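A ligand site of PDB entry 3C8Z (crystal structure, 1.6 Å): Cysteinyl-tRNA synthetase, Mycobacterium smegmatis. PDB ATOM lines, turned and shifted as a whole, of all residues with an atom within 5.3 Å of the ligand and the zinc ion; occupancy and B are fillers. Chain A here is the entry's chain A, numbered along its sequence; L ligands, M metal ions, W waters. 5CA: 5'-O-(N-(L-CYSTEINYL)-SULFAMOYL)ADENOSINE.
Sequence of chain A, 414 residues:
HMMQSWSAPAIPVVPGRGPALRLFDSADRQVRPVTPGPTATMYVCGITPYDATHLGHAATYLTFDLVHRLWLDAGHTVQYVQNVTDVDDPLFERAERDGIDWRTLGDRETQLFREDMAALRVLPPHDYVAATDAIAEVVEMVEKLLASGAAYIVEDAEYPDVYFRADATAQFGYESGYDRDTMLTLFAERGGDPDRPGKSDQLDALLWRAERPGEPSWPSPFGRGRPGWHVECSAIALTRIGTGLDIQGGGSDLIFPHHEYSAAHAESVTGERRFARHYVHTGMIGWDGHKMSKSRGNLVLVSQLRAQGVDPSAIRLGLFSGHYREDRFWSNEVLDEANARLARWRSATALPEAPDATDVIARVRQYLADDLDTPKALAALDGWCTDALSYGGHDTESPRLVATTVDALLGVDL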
ATOM      1  N   TYR A  43     -17.869 -13.578  27.519  1.00  0.00           N
ATOM      2  CA  TYR A  43     -18.106 -14.595  26.521  1.00  0.00           C
ATOM      3  C   TYR A  43     -17.690 -13.964  25.199  1.00  0.00           C
ATOM      4  O   TYR A  43     -18.147 -12.868  24.904  1.00  0.00           O
ATOM      5  CB  TYR A  43     -19.594 -14.948  26.461  1.00  0.00           C
ATOM      6  CG  TYR A  43     -19.909 -16.049  25.474  1.00  0.00           C
ATOM      7  CD1 TYR A  43     -19.981 -17.362  25.901  1.00  0.00           C
ATOM      8  CD2 TYR A  43     -20.151 -15.777  24.115  1.00  0.00           C
ATOM      9  CE1 TYR A  43     -20.250 -18.385  25.020  1.00  0.00           C
ATOM     10  CE2 TYR A  43     -20.452 -16.807  23.230  1.00  0.00           C
ATOM     11  CZ  TYR A  43     -20.497 -18.114  23.692  1.00  0.00           C
ATOM     12  OH  TYR A  43     -20.802 -19.123  22.846  1.00  0.00           O
ATOM     13  N   VAL A  44     -16.815 -14.644  24.460  1.00  0.00           N
ATOM     14  CA  VAL A  44     -16.370 -14.171  23.161  1.00  0.00           C
ATOM     15  C   VAL A  44     -16.676 -15.243  22.129  1.00  0.00           C
ATOM     16  O   VAL A  44     -16.292 -16.400  22.299  1.00  0.00           O
ATOM     17  CB  VAL A  44     -14.891 -13.778  23.127  1.00  0.00           C
ATOM     18  CG1 VAL A  44     -14.464 -13.379  21.697  1.00  0.00           C
ATOM     19  CG2 VAL A  44     -14.601 -12.645  24.144  1.00  0.00           C
ATOM     20  N   CYS A  45     -17.350 -14.864  21.064  1.00  0.00           N
ATOM     21  CA  CYS A  45     -17.729 -15.829  20.050  1.00  0.00           C
ATOM     22  C   CYS A  45     -16.504 -16.421  19.363  1.00  0.00           C
ATOM     23  O   CYS A  45     -15.662 -15.707  18.823  1.00  0.00           O
ATOM     24  CB  CYS A  45     -18.683 -15.187  19.036  1.00  0.00           C
ATOM     25  SG  CYS A  45     -20.330 -14.996  19.668  1.00  0.00           S
ATOM     26  N   GLY A  46     -16.447 -17.747  19.416  1.00  0.00           N
ATOM     27  CA  GLY A  46     -15.315 -18.543  18.938  1.00  0.00           C
ATOM     28  C   GLY A  46     -15.333 -18.841  17.450  1.00  0.00           C
ATOM     29  O   GLY A  46     -16.148 -18.294  16.701  1.00  0.00           O
ATOM     30  N   ILE A  47     -14.445 -19.728  17.017  1.00  0.00           N
ATOM     31  CA  ILE A  47     -14.307 -19.986  15.594  1.00  0.00           C
ATOM     32  C   ILE A  47     -15.306 -21.024  15.095  1.00  0.00           C
ATOM     33  O   ILE A  47     -15.823 -21.839  15.863  1.00  0.00           O
ATOM     34  CB  ILE A  47     -12.873 -20.430  15.194  1.00  0.00           C
ATOM     35  CG1 ILE A  47     -12.500 -21.768  15.854  1.00  0.00           C
ATOM     36  CG2 ILE A  47     -11.884 -19.310  15.492  1.00  0.00           C
ATOM     37  CD1 ILE A  47     -11.291 -22.440  15.198  1.00  0.00           C
ATOM     38  N   THR A  48     -15.583 -20.948  13.794  1.00  0.00           N
ATOM     39  CA  THR A  48     -16.181 -22.064  13.053  1.00  0.00           C
ATOM     40  C   THR A  48     -15.020 -22.766  12.366  1.00  0.00           C
ATOM     41  O   THR A  48     -14.402 -22.211  11.440  1.00  0.00           O
ATOM     42  CB  THR A  48     -17.207 -21.559  12.034  1.00  0.00           C
ATOM     43  OG1 THR A  48     -18.259 -20.885  12.707  1.00  0.00           O
ATOM     44  CG2 THR A  48     -17.815 -22.740  11.281  1.00  0.00           C
ATOM     45  N   HIS A  54      -7.048 -16.990  10.379  1.00  0.00           N
ATOM     46  CA  HIS A  54      -6.481 -15.812   9.765  1.00  0.00           C
ATOM     47  C   HIS A  54      -6.282 -14.644  10.679  1.00  0.00           C
ATOM     48  O   HIS A  54      -6.658 -14.704  11.808  1.00  0.00           O
ATOM     49  CB  HIS A  54      -7.165 -15.423   8.456  1.00  0.00           C
ATOM     50  CG  HIS A  54      -8.587 -15.014   8.593  1.00  0.00           C
ATOM     51  ND1 HIS A  54      -8.977 -13.975   9.394  1.00  0.00           N
ATOM     52  CD2 HIS A  54      -9.701 -15.468   7.992  1.00  0.00           C
ATOM     53  CE1 HIS A  54     -10.271 -13.823   9.288  1.00  0.00           C
ATOM     54  NE2 HIS A  54     -10.734 -14.694   8.428  1.00  0.00           N
ATOM     55  N   GLY A  56      -7.506 -11.798  10.893  1.00  0.00           N
ATOM     56  CA  GLY A  56      -8.765 -11.338  11.377  1.00  0.00           C
ATOM     57  C   GLY A  56      -9.222 -11.995  12.658  1.00  0.00           C
ATOM     58  O   GLY A  56      -9.515 -11.305  13.586  1.00  0.00           O
ATOM     59  N   HIS A  57      -9.334 -13.321  12.644  1.00  0.00           N
ATOM     60  CA  HIS A  57      -9.670 -13.976  13.876  1.00  0.00           C
ATOM     61  C   HIS A  57      -8.676 -13.605  14.961  1.00  0.00           C
ATOM     62  O   HIS A  57      -9.075 -13.316  16.084  1.00  0.00           O
ATOM     63  CB  HIS A  57      -9.585 -15.479  13.671  1.00  0.00           C
ATOM     64  CG  HIS A  57     -10.317 -15.973  12.461  1.00  0.00           C
ATOM     65  ND1 HIS A  57     -11.650 -15.719  12.237  1.00  0.00           N
ATOM     66  CD2 HIS A  57      -9.901 -16.743  11.432  1.00  0.00           C
ATOM     67  CE1 HIS A  57     -12.026 -16.297  11.118  1.00  0.00           C
ATOM     68  NE2 HIS A  57     -10.989 -16.929  10.604  1.00  0.00           N
ATOM     69  N   ALA A  59      -6.762 -10.938  15.364  1.00  0.00           N
ATOM     70  CA  ALA A  59      -6.973  -9.586  15.889  1.00  0.00           C
ATOM     71  C   ALA A  59      -8.119  -9.524  16.881  1.00  0.00           C
ATOM     72  O   ALA A  59      -8.040  -8.861  17.912  1.00  0.00           O
ATOM     73  CB  ALA A  59      -7.188  -8.610  14.771  1.00  0.00           C
ATOM     74  N   THR A  60      -9.209 -10.226  16.580  1.00  0.00           N
ATOM     75  CA  THR A  60     -10.344 -10.254  17.479  1.00  0.00           C
ATOM     76  C   THR A  60      -9.997 -10.897  18.825  1.00  0.00           C
ATOM     77  O   THR A  60     -10.262 -10.292  19.861  1.00  0.00           O
ATOM     78  CB  THR A  60     -11.538 -10.901  16.790  1.00  0.00           C
ATOM     79  OG1 THR A  60     -11.990  -9.985  15.784  1.00  0.00           O
ATOM     80  CG2 THR A  60     -12.674 -11.185  17.790  1.00  0.00           C
ATOM     81  N   TYR A  61      -9.348 -12.060  18.825  1.00  0.00           N
ATOM     82  CA  TYR A  61      -9.029 -12.698  20.114  1.00  0.00           C
ATOM     83  C   TYR A  61      -7.935 -11.958  20.878  1.00  0.00           C
ATOM     84  O   TYR A  61      -7.948 -11.956  22.100  1.00  0.00           O
ATOM     85  CB  TYR A  61      -8.733 -14.199  19.950  1.00  0.00           C
ATOM     86  CG  TYR A  61      -9.934 -14.860  19.355  1.00  0.00           C
ATOM     87  CD1 TYR A  61     -11.138 -14.900  20.062  1.00  0.00           C
ATOM     88  CD2 TYR A  61      -9.902 -15.368  18.057  1.00  0.00           C
ATOM     89  CE1 TYR A  61     -12.292 -15.472  19.501  1.00  0.00           C
ATOM     90  CE2 TYR A  61     -11.047 -15.923  17.472  1.00  0.00           C
ATOM     91  CZ  TYR A  61     -12.228 -15.972  18.207  1.00  0.00           C
ATOM     92  OH  TYR A  61     -13.347 -16.512  17.617  1.00  0.00           O
ATOM     93  N   ASN A  83     -16.837 -20.469  22.745  1.00  0.00           N
ATOM     94  CA  ASN A  83     -17.373 -21.673  22.097  1.00  0.00           C
ATOM     95  C   ASN A  83     -16.532 -22.093  20.886  1.00  0.00           C
ATOM     96  O   ASN A  83     -15.606 -21.393  20.478  1.00  0.00           O
ATOM     97  CB  ASN A  83     -18.791 -21.360  21.594  1.00  0.00           C
ATOM     98  CG  ASN A  83     -18.793 -20.239  20.550  1.00  0.00           C
ATOM     99  OD1 ASN A  83     -18.309 -19.136  20.831  1.00  0.00           O
ATOM    100  ND2 ASN A  83     -19.281 -20.524  19.351  1.00  0.00           N
ATOM    101  N   THR A  85     -18.015 -23.376  17.098  1.00  0.00           N
ATOM    102  CA  THR A  85     -19.200 -23.704  16.300  1.00  0.00           C
ATOM    103  C   THR A  85     -18.839 -24.891  15.389  1.00  0.00           C
ATOM    104  O   THR A  85     -18.578 -24.728  14.183  1.00  0.00           O
ATOM    105  CB  THR A  85     -19.707 -22.463  15.518  1.00  0.00           C
ATOM    106  OG1 THR A  85     -19.817 -21.355  16.433  1.00  0.00           O
ATOM    107  CG2 THR A  85     -21.067 -22.752  14.903  1.00  0.00           C
ATOM    108  N   TRP A 229     -27.959 -21.219  15.099  1.00  0.00           N
ATOM    109  CA  TRP A 229     -26.679 -20.645  15.479  1.00  0.00           C
ATOM    110  C   TRP A 229     -26.752 -19.787  16.743  1.00  0.00           C
ATOM    111  O   TRP A 229     -25.943 -19.934  17.660  1.00  0.00           O
ATOM    112  CB  TRP A 229     -26.154 -19.837  14.283  1.00  0.00           C
ATOM    113  CG  TRP A 229     -24.863 -19.143  14.505  1.00  0.00           C
ATOM    114  CD1 TRP A 229     -23.854 -19.498  15.367  1.00  0.00           C
ATOM    115  CD2 TRP A 229     -24.421 -17.950  13.846  1.00  0.00           C
ATOM    116  NE1 TRP A 229     -22.822 -18.584  15.285  1.00  0.00           N
ATOM    117  CE2 TRP A 229     -23.152 -17.626  14.358  1.00  0.00           C
ATOM    118  CE3 TRP A 229     -24.986 -17.114  12.865  1.00  0.00           C
ATOM    119  CZ2 TRP A 229     -22.425 -16.510  13.921  1.00  0.00           C
ATOM    120  CZ3 TRP A 229     -24.271 -15.993  12.439  1.00  0.00           C
ATOM    121  CH2 TRP A 229     -23.010 -15.709  12.967  1.00  0.00           C
ATOM    122  N   CYS A 233     -24.819 -20.076  21.165  1.00  0.00           N
ATOM    123  CA  CYS A 233     -24.059 -19.141  21.985  1.00  0.00           C
ATOM    124  C   CYS A 233     -24.839 -18.625  23.197  1.00  0.00           C
ATOM    125  O   CYS A 233     -24.282 -18.453  24.287  1.00  0.00           O
ATOM    126  CB  CYS A 233     -23.460 -18.009  21.107  1.00  0.00           C
ATOM    127  SG  CYS A 233     -22.207 -18.630  20.022  1.00  0.00           S
ATOM    128  N   GLY A 249     -18.601 -10.473  23.483  1.00  0.00           N
ATOM    129  CA  GLY A 249     -17.669  -9.973  22.478  1.00  0.00           C
ATOM    130  C   GLY A 249     -17.618 -10.752  21.167  1.00  0.00           C
ATOM    131  O   GLY A 249     -18.013 -11.924  21.105  1.00  0.00           O
ATOM    132  N   GLY A 250     -17.111 -10.093  20.133  1.00  0.00           N
ATOM    133  CA  GLY A 250     -16.764 -10.736  18.866  1.00  0.00           C
ATOM    134  C   GLY A 250     -16.536  -9.685  17.807  1.00  0.00           C
ATOM    135  O   GLY A 250     -16.422  -8.501  18.152  1.00  0.00           O
ATOM    136  N   GLY A 251     -16.464 -10.108  16.554  1.00  0.00           N
ATOM    137  CA  GLY A 251     -16.291  -9.163  15.434  1.00  0.00           C
ATOM    138  C   GLY A 251     -17.563  -8.402  15.163  1.00  0.00           C
ATOM    139  O   GLY A 251     -18.660  -8.832  15.543  1.00  0.00           O
ATOM    140  N   SER A 252     -17.423  -7.229  14.540  1.00  0.00           N
ATOM    141  CA  SER A 252     -18.543  -6.365  14.215  1.00  0.00           C
ATOM    142  C   SER A 252     -19.587  -7.008  13.290  1.00  0.00           C
ATOM    143  O   SER A 252     -20.760  -6.589  13.340  1.00  0.00           O
ATOM    144  CB  SER A 252     -18.040  -5.049  13.635  1.00  0.00           C
ATOM    145  OG  SER A 252     -17.521  -4.245  14.677  1.00  0.00           O
ATOM    146  N   ASP A 253     -19.189  -8.028  12.527  1.00  0.00           N
ATOM    147  CA  ASP A 253     -20.144  -8.767  11.692  1.00  0.00           C
ATOM    148  C   ASP A 253     -21.203  -9.501  12.550  1.00  0.00           C
ATOM    149  O   ASP A 253     -22.262  -9.872  12.054  1.00  0.00           O
ATOM    150  CB  ASP A 253     -19.437  -9.755  10.738  1.00  0.00           C
ATOM    151  CG  ASP A 253     -18.700 -10.856  11.491  1.00  0.00           C
ATOM    152  OD1 ASP A 253     -17.895 -10.537  12.376  1.00  0.00           O
ATOM    153  OD2 ASP A 253     -18.995 -12.043  11.183  1.00  0.00           O
ATOM    154  N   LEU A 254     -20.900  -9.703  13.831  1.00  0.00           N
ATOM    155  CA  LEU A 254     -21.839 -10.385  14.736  1.00  0.00           C
ATOM    156  C   LEU A 254     -22.861  -9.470  15.398  1.00  0.00           C
ATOM    157  O   LEU A 254     -23.775  -9.930  16.102  1.00  0.00           O
ATOM    158  CB  LEU A 254     -21.050 -11.187  15.803  1.00  0.00           C
ATOM    159  CG  LEU A 254     -20.066 -12.206  15.220  1.00  0.00           C
ATOM    160  CD1 LEU A 254     -19.365 -12.906  16.390  1.00  0.00           C
ATOM    161  CD2 LEU A 254     -20.766 -13.224  14.340  1.00  0.00           C
ATOM    162  N   HIS A 258     -26.400 -12.048  14.833  1.00  0.00           N
ATOM    163  CA  HIS A 258     -26.033 -13.016  15.847  1.00  0.00           C
ATOM    164  C   HIS A 258     -26.228 -12.544  17.336  1.00  0.00           C
ATOM    165  O   HIS A 258     -26.871 -13.154  18.099  1.00  0.00           O
ATOM    166  CB  HIS A 258     -24.615 -13.454  15.612  1.00  0.00           C
ATOM    167  CG  HIS A 258     -24.168 -14.588  16.472  1.00  0.00           C
ATOM    168  ND1 HIS A 258     -24.868 -15.767  16.577  1.00  0.00           N
ATOM    169  CD2 HIS A 258     -23.073 -14.729  17.236  1.00  0.00           C
ATOM    170  CE1 HIS A 258     -24.218 -16.567  17.389  1.00  0.00           C
ATOM    171  NE2 HIS A 258     -23.146 -15.956  17.795  1.00  0.00           N
ATOM    172  N   HIS A 259     -25.597 -11.442  17.688  1.00  0.00           N
ATOM    173  CA  HIS A 259     -25.643 -10.965  19.053  1.00  0.00           C
ATOM    174  C   HIS A 259     -27.011 -10.409  19.470  1.00  0.00           C
ATOM    175  O   HIS A 259     -27.403 -10.478  20.613  1.00  0.00           O
ATOM    176  CB  HIS A 259     -24.552  -9.923  19.274  1.00  0.00           C
ATOM    177  CG  HIS A 259     -23.199 -10.522  19.331  1.00  0.00           C
ATOM    178  ND1 HIS A 259     -22.044  -9.788  19.365  1.00  0.00           N
ATOM    179  CD2 HIS A 259     -22.820 -11.815  19.365  1.00  0.00           C
ATOM    180  CE1 HIS A 259     -21.026 -10.605  19.404  1.00  0.00           C
ATOM    181  NE2 HIS A 259     -21.463 -11.837  19.416  1.00  0.00           N
ATOM    182  N   THR A 282     -15.087  -5.827  17.651  1.00  0.00           N
ATOM    183  CA  THR A 282     -13.841  -5.466  16.993  1.00  0.00           C
ATOM    184  C   THR A 282     -14.056  -5.097  15.537  1.00  0.00           C
ATOM    185  O   THR A 282     -15.016  -5.552  14.874  1.00  0.00           O
ATOM    186  CB  THR A 282     -12.847  -6.626  17.055  1.00  0.00           C
ATOM    187  OG1 THR A 282     -13.514  -7.800  16.605  1.00  0.00           O
ATOM    188  CG2 THR A 282     -12.357  -6.815  18.470  1.00  0.00           C
ATOM    189  N   GLY A 283     -13.130  -4.295  15.027  1.00  0.00           N
ATOM    190  CA  GLY A 283     -13.087  -3.966  13.610  1.00  0.00           C
ATOM    191  C   GLY A 283     -12.693  -5.144  12.764  1.00  0.00           C
ATOM    192  O   GLY A 283     -12.095  -6.138  13.229  1.00  0.00           O
ATOM    193  N   MET A 284     -13.002  -5.051  11.475  1.00  0.00           N
ATOM    194  CA  MET A 284     -12.707  -6.127  10.571  1.00  0.00           C
ATOM    195  C   MET A 284     -11.324  -5.916   9.961  1.00  0.00           C
ATOM    196  O   MET A 284     -10.981  -4.788   9.547  1.00  0.00           O
ATOM    197  CB  MET A 284     -13.827  -6.221   9.523  1.00  0.00           C
ATOM    198  CG  MET A 284     -15.233  -6.388  10.151  1.00  0.00           C
ATOM    199  SD  MET A 284     -15.491  -7.881  11.205  1.00  0.00           S
ATOM    200  CE  MET A 284     -15.527  -9.030   9.878  1.00  0.00           C
ATOM    201  N   ILE A 285     -10.511  -6.978   9.956  1.00  0.00           N
ATOM    202  CA  ILE A 285      -9.186  -6.955   9.315  1.00  0.00           C
ATOM    203  C   ILE A 285      -9.316  -7.426   7.873  1.00  0.00           C
ATOM    204  O   ILE A 285      -9.998  -8.416   7.597  1.00  0.00           O
ATOM    205  CB  ILE A 285      -8.176  -7.864  10.058  1.00  0.00           C
ATOM    206  CG1 ILE A 285      -8.147  -7.524  11.550  1.00  0.00           C
ATOM    207  CG2 ILE A 285      -6.754  -7.734   9.451  1.00  0.00           C
ATOM    208  CD1 ILE A 285      -7.744  -6.082  11.864  1.00  0.00           C
HETATM  209  N   5CA L   1     -18.427 -19.327  15.074  1.00  0.00           N
HETATM  210  CA  5CA L   1     -18.502 -17.848  15.036  1.00  0.00           C
HETATM  211  CB  5CA L   1     -19.334 -17.066  15.991  1.00  0.00           C
HETATM  212  SG  5CA L   1     -20.154 -18.125  17.207  1.00  0.00           S
HETATM  213  C   5CA L   1     -17.904 -17.124  13.890  1.00  0.00           C
HETATM  214  O   5CA L   1     -18.275 -16.038  13.411  1.00  0.00           O
HETATM  215  N3S 5CA L   1     -16.786 -17.758  13.639  1.00  0.00           N
HETATM  216  S   5CA L   1     -15.712 -17.267  12.604  1.00  0.00           S
HETATM  217  O1S 5CA L   1     -16.328 -16.905  11.309  1.00  0.00           O
HETATM  218  O2S 5CA L   1     -14.626 -18.280  12.514  1.00  0.00           O
HETATM  219  O5' 5CA L   1     -15.162 -16.042  13.258  1.00  0.00           O
HETATM  220  C5' 5CA L   1     -14.497 -16.102  14.583  1.00  0.00           C
HETATM  221  C4' 5CA L   1     -14.594 -14.676  14.849  1.00  0.00           C
HETATM  222  O4' 5CA L   1     -13.639 -13.796  14.366  1.00  0.00           O
HETATM  223  C3' 5CA L   1     -15.605 -13.729  15.546  1.00  0.00           C
HETATM  224  O3' 5CA L   1     -15.783 -13.242  16.767  1.00  0.00           O
HETATM  225  C2' 5CA L   1     -15.949 -13.021  14.345  1.00  0.00           C
HETATM  226  O2' 5CA L   1     -16.833 -11.942  14.449  1.00  0.00           O
HETATM  227  C1' 5CA L   1     -14.486 -12.613  13.996  1.00  0.00           C
HETATM  228  N9  5CA L   1     -14.156 -12.340  12.646  1.00  0.00           N
HETATM  229  C8  5CA L   1     -14.499 -12.946  11.494  1.00  0.00           C
HETATM  230  N7  5CA L   1     -13.886 -12.399  10.407  1.00  0.00           N
HETATM  231  C5  5CA L   1     -13.087 -11.341  10.922  1.00  0.00           C
HETATM  232  C6  5CA L   1     -12.162 -10.356  10.258  1.00  0.00           C
HETATM  233  N6  5CA L   1     -12.022 -10.353   8.926  1.00  0.00           N
HETATM  234  N1  5CA L   1     -11.560  -9.434  11.133  1.00  0.00           N
HETATM  235  C2  5CA L   1     -11.749  -9.430  12.543  1.00  0.00           C
HETATM  236  N3  5CA L   1     -12.584 -10.349  13.196  1.00  0.00           N
HETATM  237  C4  5CA L   1     -13.248 -11.321  12.336  1.00  0.00           C
HETATM  238 ZN    ZN M   1     -21.451 -16.789  18.785  1.00  0.00          ZN
HETATM  239  O   HOH W   1     -12.953 -11.898   6.798  1.00  0.00           O
HETATM  240  O   HOH W   2     -16.470 -12.218   8.531  1.00  0.00           O
HETATM  241  O   HOH W   3     -16.490 -14.717   9.056  1.00  0.00           O
HETATM  242  O   HOH W   4     -13.509 -19.691  10.492  1.00  0.00           O
HETATM  243  O   HOH W   5     -14.083 -15.905   8.969  1.00  0.00           O
HETATM  244  O   HOH W   6     -10.387  -7.507  14.921  1.00  0.00           O
HETATM  245  O   HOH W   7     -17.872 -14.316  11.466  1.00  0.00           O
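A nitrogen (N1) of the ligand sits at hydrogen-bond distance from the backbone NH (N) of Ile 285, at 2.9 Å.
A nitrogen (N) of the ligand lies within hydrogen-bond range of the side-chain hydroxyl (OG1) of Thr 85.
OG1 of Thr 48 lies within hydrogen-bond range of N of the ligand (2.8 Å).
The backbone carbonyl oxygen (O) of Ile 285 is in hydrogen-bond range of a nitrogen (N6) of the ligand (3.1 Å).
A nitrogen (N) of the ligand lies close to the backbone carbonyl oxygen (O) of Gly 46 (3.0 Å).
An oxygen (O3') of the ligand sits at hydrogen-bond distance from the backbone carbonyl oxygen (O) of Cys 45, 3.2 Å away.
OG1 of Thr 60 is in hydrogen-bond range of N3 of the ligand (2.7 Å).
A ring nitrogen (ND1) of His 57 lies within hydrogen-bond range of an oxygen (O4') of the ligand, 3.5 Å away.
The side-chain carboxylate (OD1) of Asp 253 lies within hydrogen-bond range of an oxygen (O2') of the ligand, 2.7 Å away.
N of Thr 48 lies within hydrogen-bond range of O2S of the ligand.
SG of the ligand sits close to NE1 of Trp 229.
A sulfur (SG) of the ligand lies close to the side-chain amide nitrogen (ND2) of Asn 83, at 3.3 Å.
An oxygen (O2') of the ligand sits at hydrogen-bond distance from the backbone NH (N) of Gly 251 (2.8 Å).
N of Gly 46 lies within hydrogen-bond range of OD1 of Asn 83.
The side-chain hydroxyl (OG1) of Thr 85 is in hydrogen-bond range of the side-chain amide nitrogen (ND2) of Asn 83 (3.1 Å).
The backbone carbonyl oxygen (O) of Gly 46 lies close to the side-chain hydroxyl (OH) of Tyr 61, at 3.4 Å.
SG of Cys 45 lies close to NE2 of His 259 (3.4 Å).
OH of Tyr 61 sits at hydrogen-bond distance from O of Cys 45, 2.7 Å away.
The backbone NH of Gly 56 is in hydrogen-bond range of a ring nitrogen (ND1) of His 54 (3.0 Å).
ND2 of Asn 83 lies close to SG of Cys 233.
The side-chain hydroxyl (OH) of Tyr 43 sits at hydrogen-bond distance from the side-chain amide oxygen (OD1) of Asn 83, at 3.2 Å.
The backbone carbonyl oxygen (O) of Gly 56 sits close to a nitrogen (N3) of the ligand, at 3.2 Å.
Residues that only touch the ligand: Tyr 61, Leu 254, Gly 283, Gly 250, Met 284, Ile 47 and His 54.
Hydrophobic or aromatic side chains within 4 Å of the ligand: Ile 47, His 54, His 57, Trp 229, Leu 254, Met 284 and Ile 285.
Of the 28 residues printed, 21 come within 4 Å of the ligand.
The nearest printed residue that does not touch the ligand is Thr 282 (4.4 Å).
Within 4 Å of the zinc ion: Cys 45, Cys 233 and His 258.
A ring nitrogen (NE2) of His 258 is bound to the zinc ion (2.1 Å).
SG of Cys 45 binds the zinc ion (2.3 Å).
SG of Cys 233 binds the zinc ion, 2.3 Å away.
A sulfur (SG) of the ligand binds the zinc ion, 2.4 Å away.
The zinc ion has four donor atoms within binding distance.
Water W7 bridges OD2 of Asp 253 and O of the ligand.
Water W4 lies within hydrogen-bond range of an oxygen (O2S) of the ligand and the backbone carbonyl oxygen (O) of Thr 48.
Water W6 lies within hydrogen-bond range of O of Gly 283 (2.8 Å) and OG1 of Thr 60 (3.1 Å).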
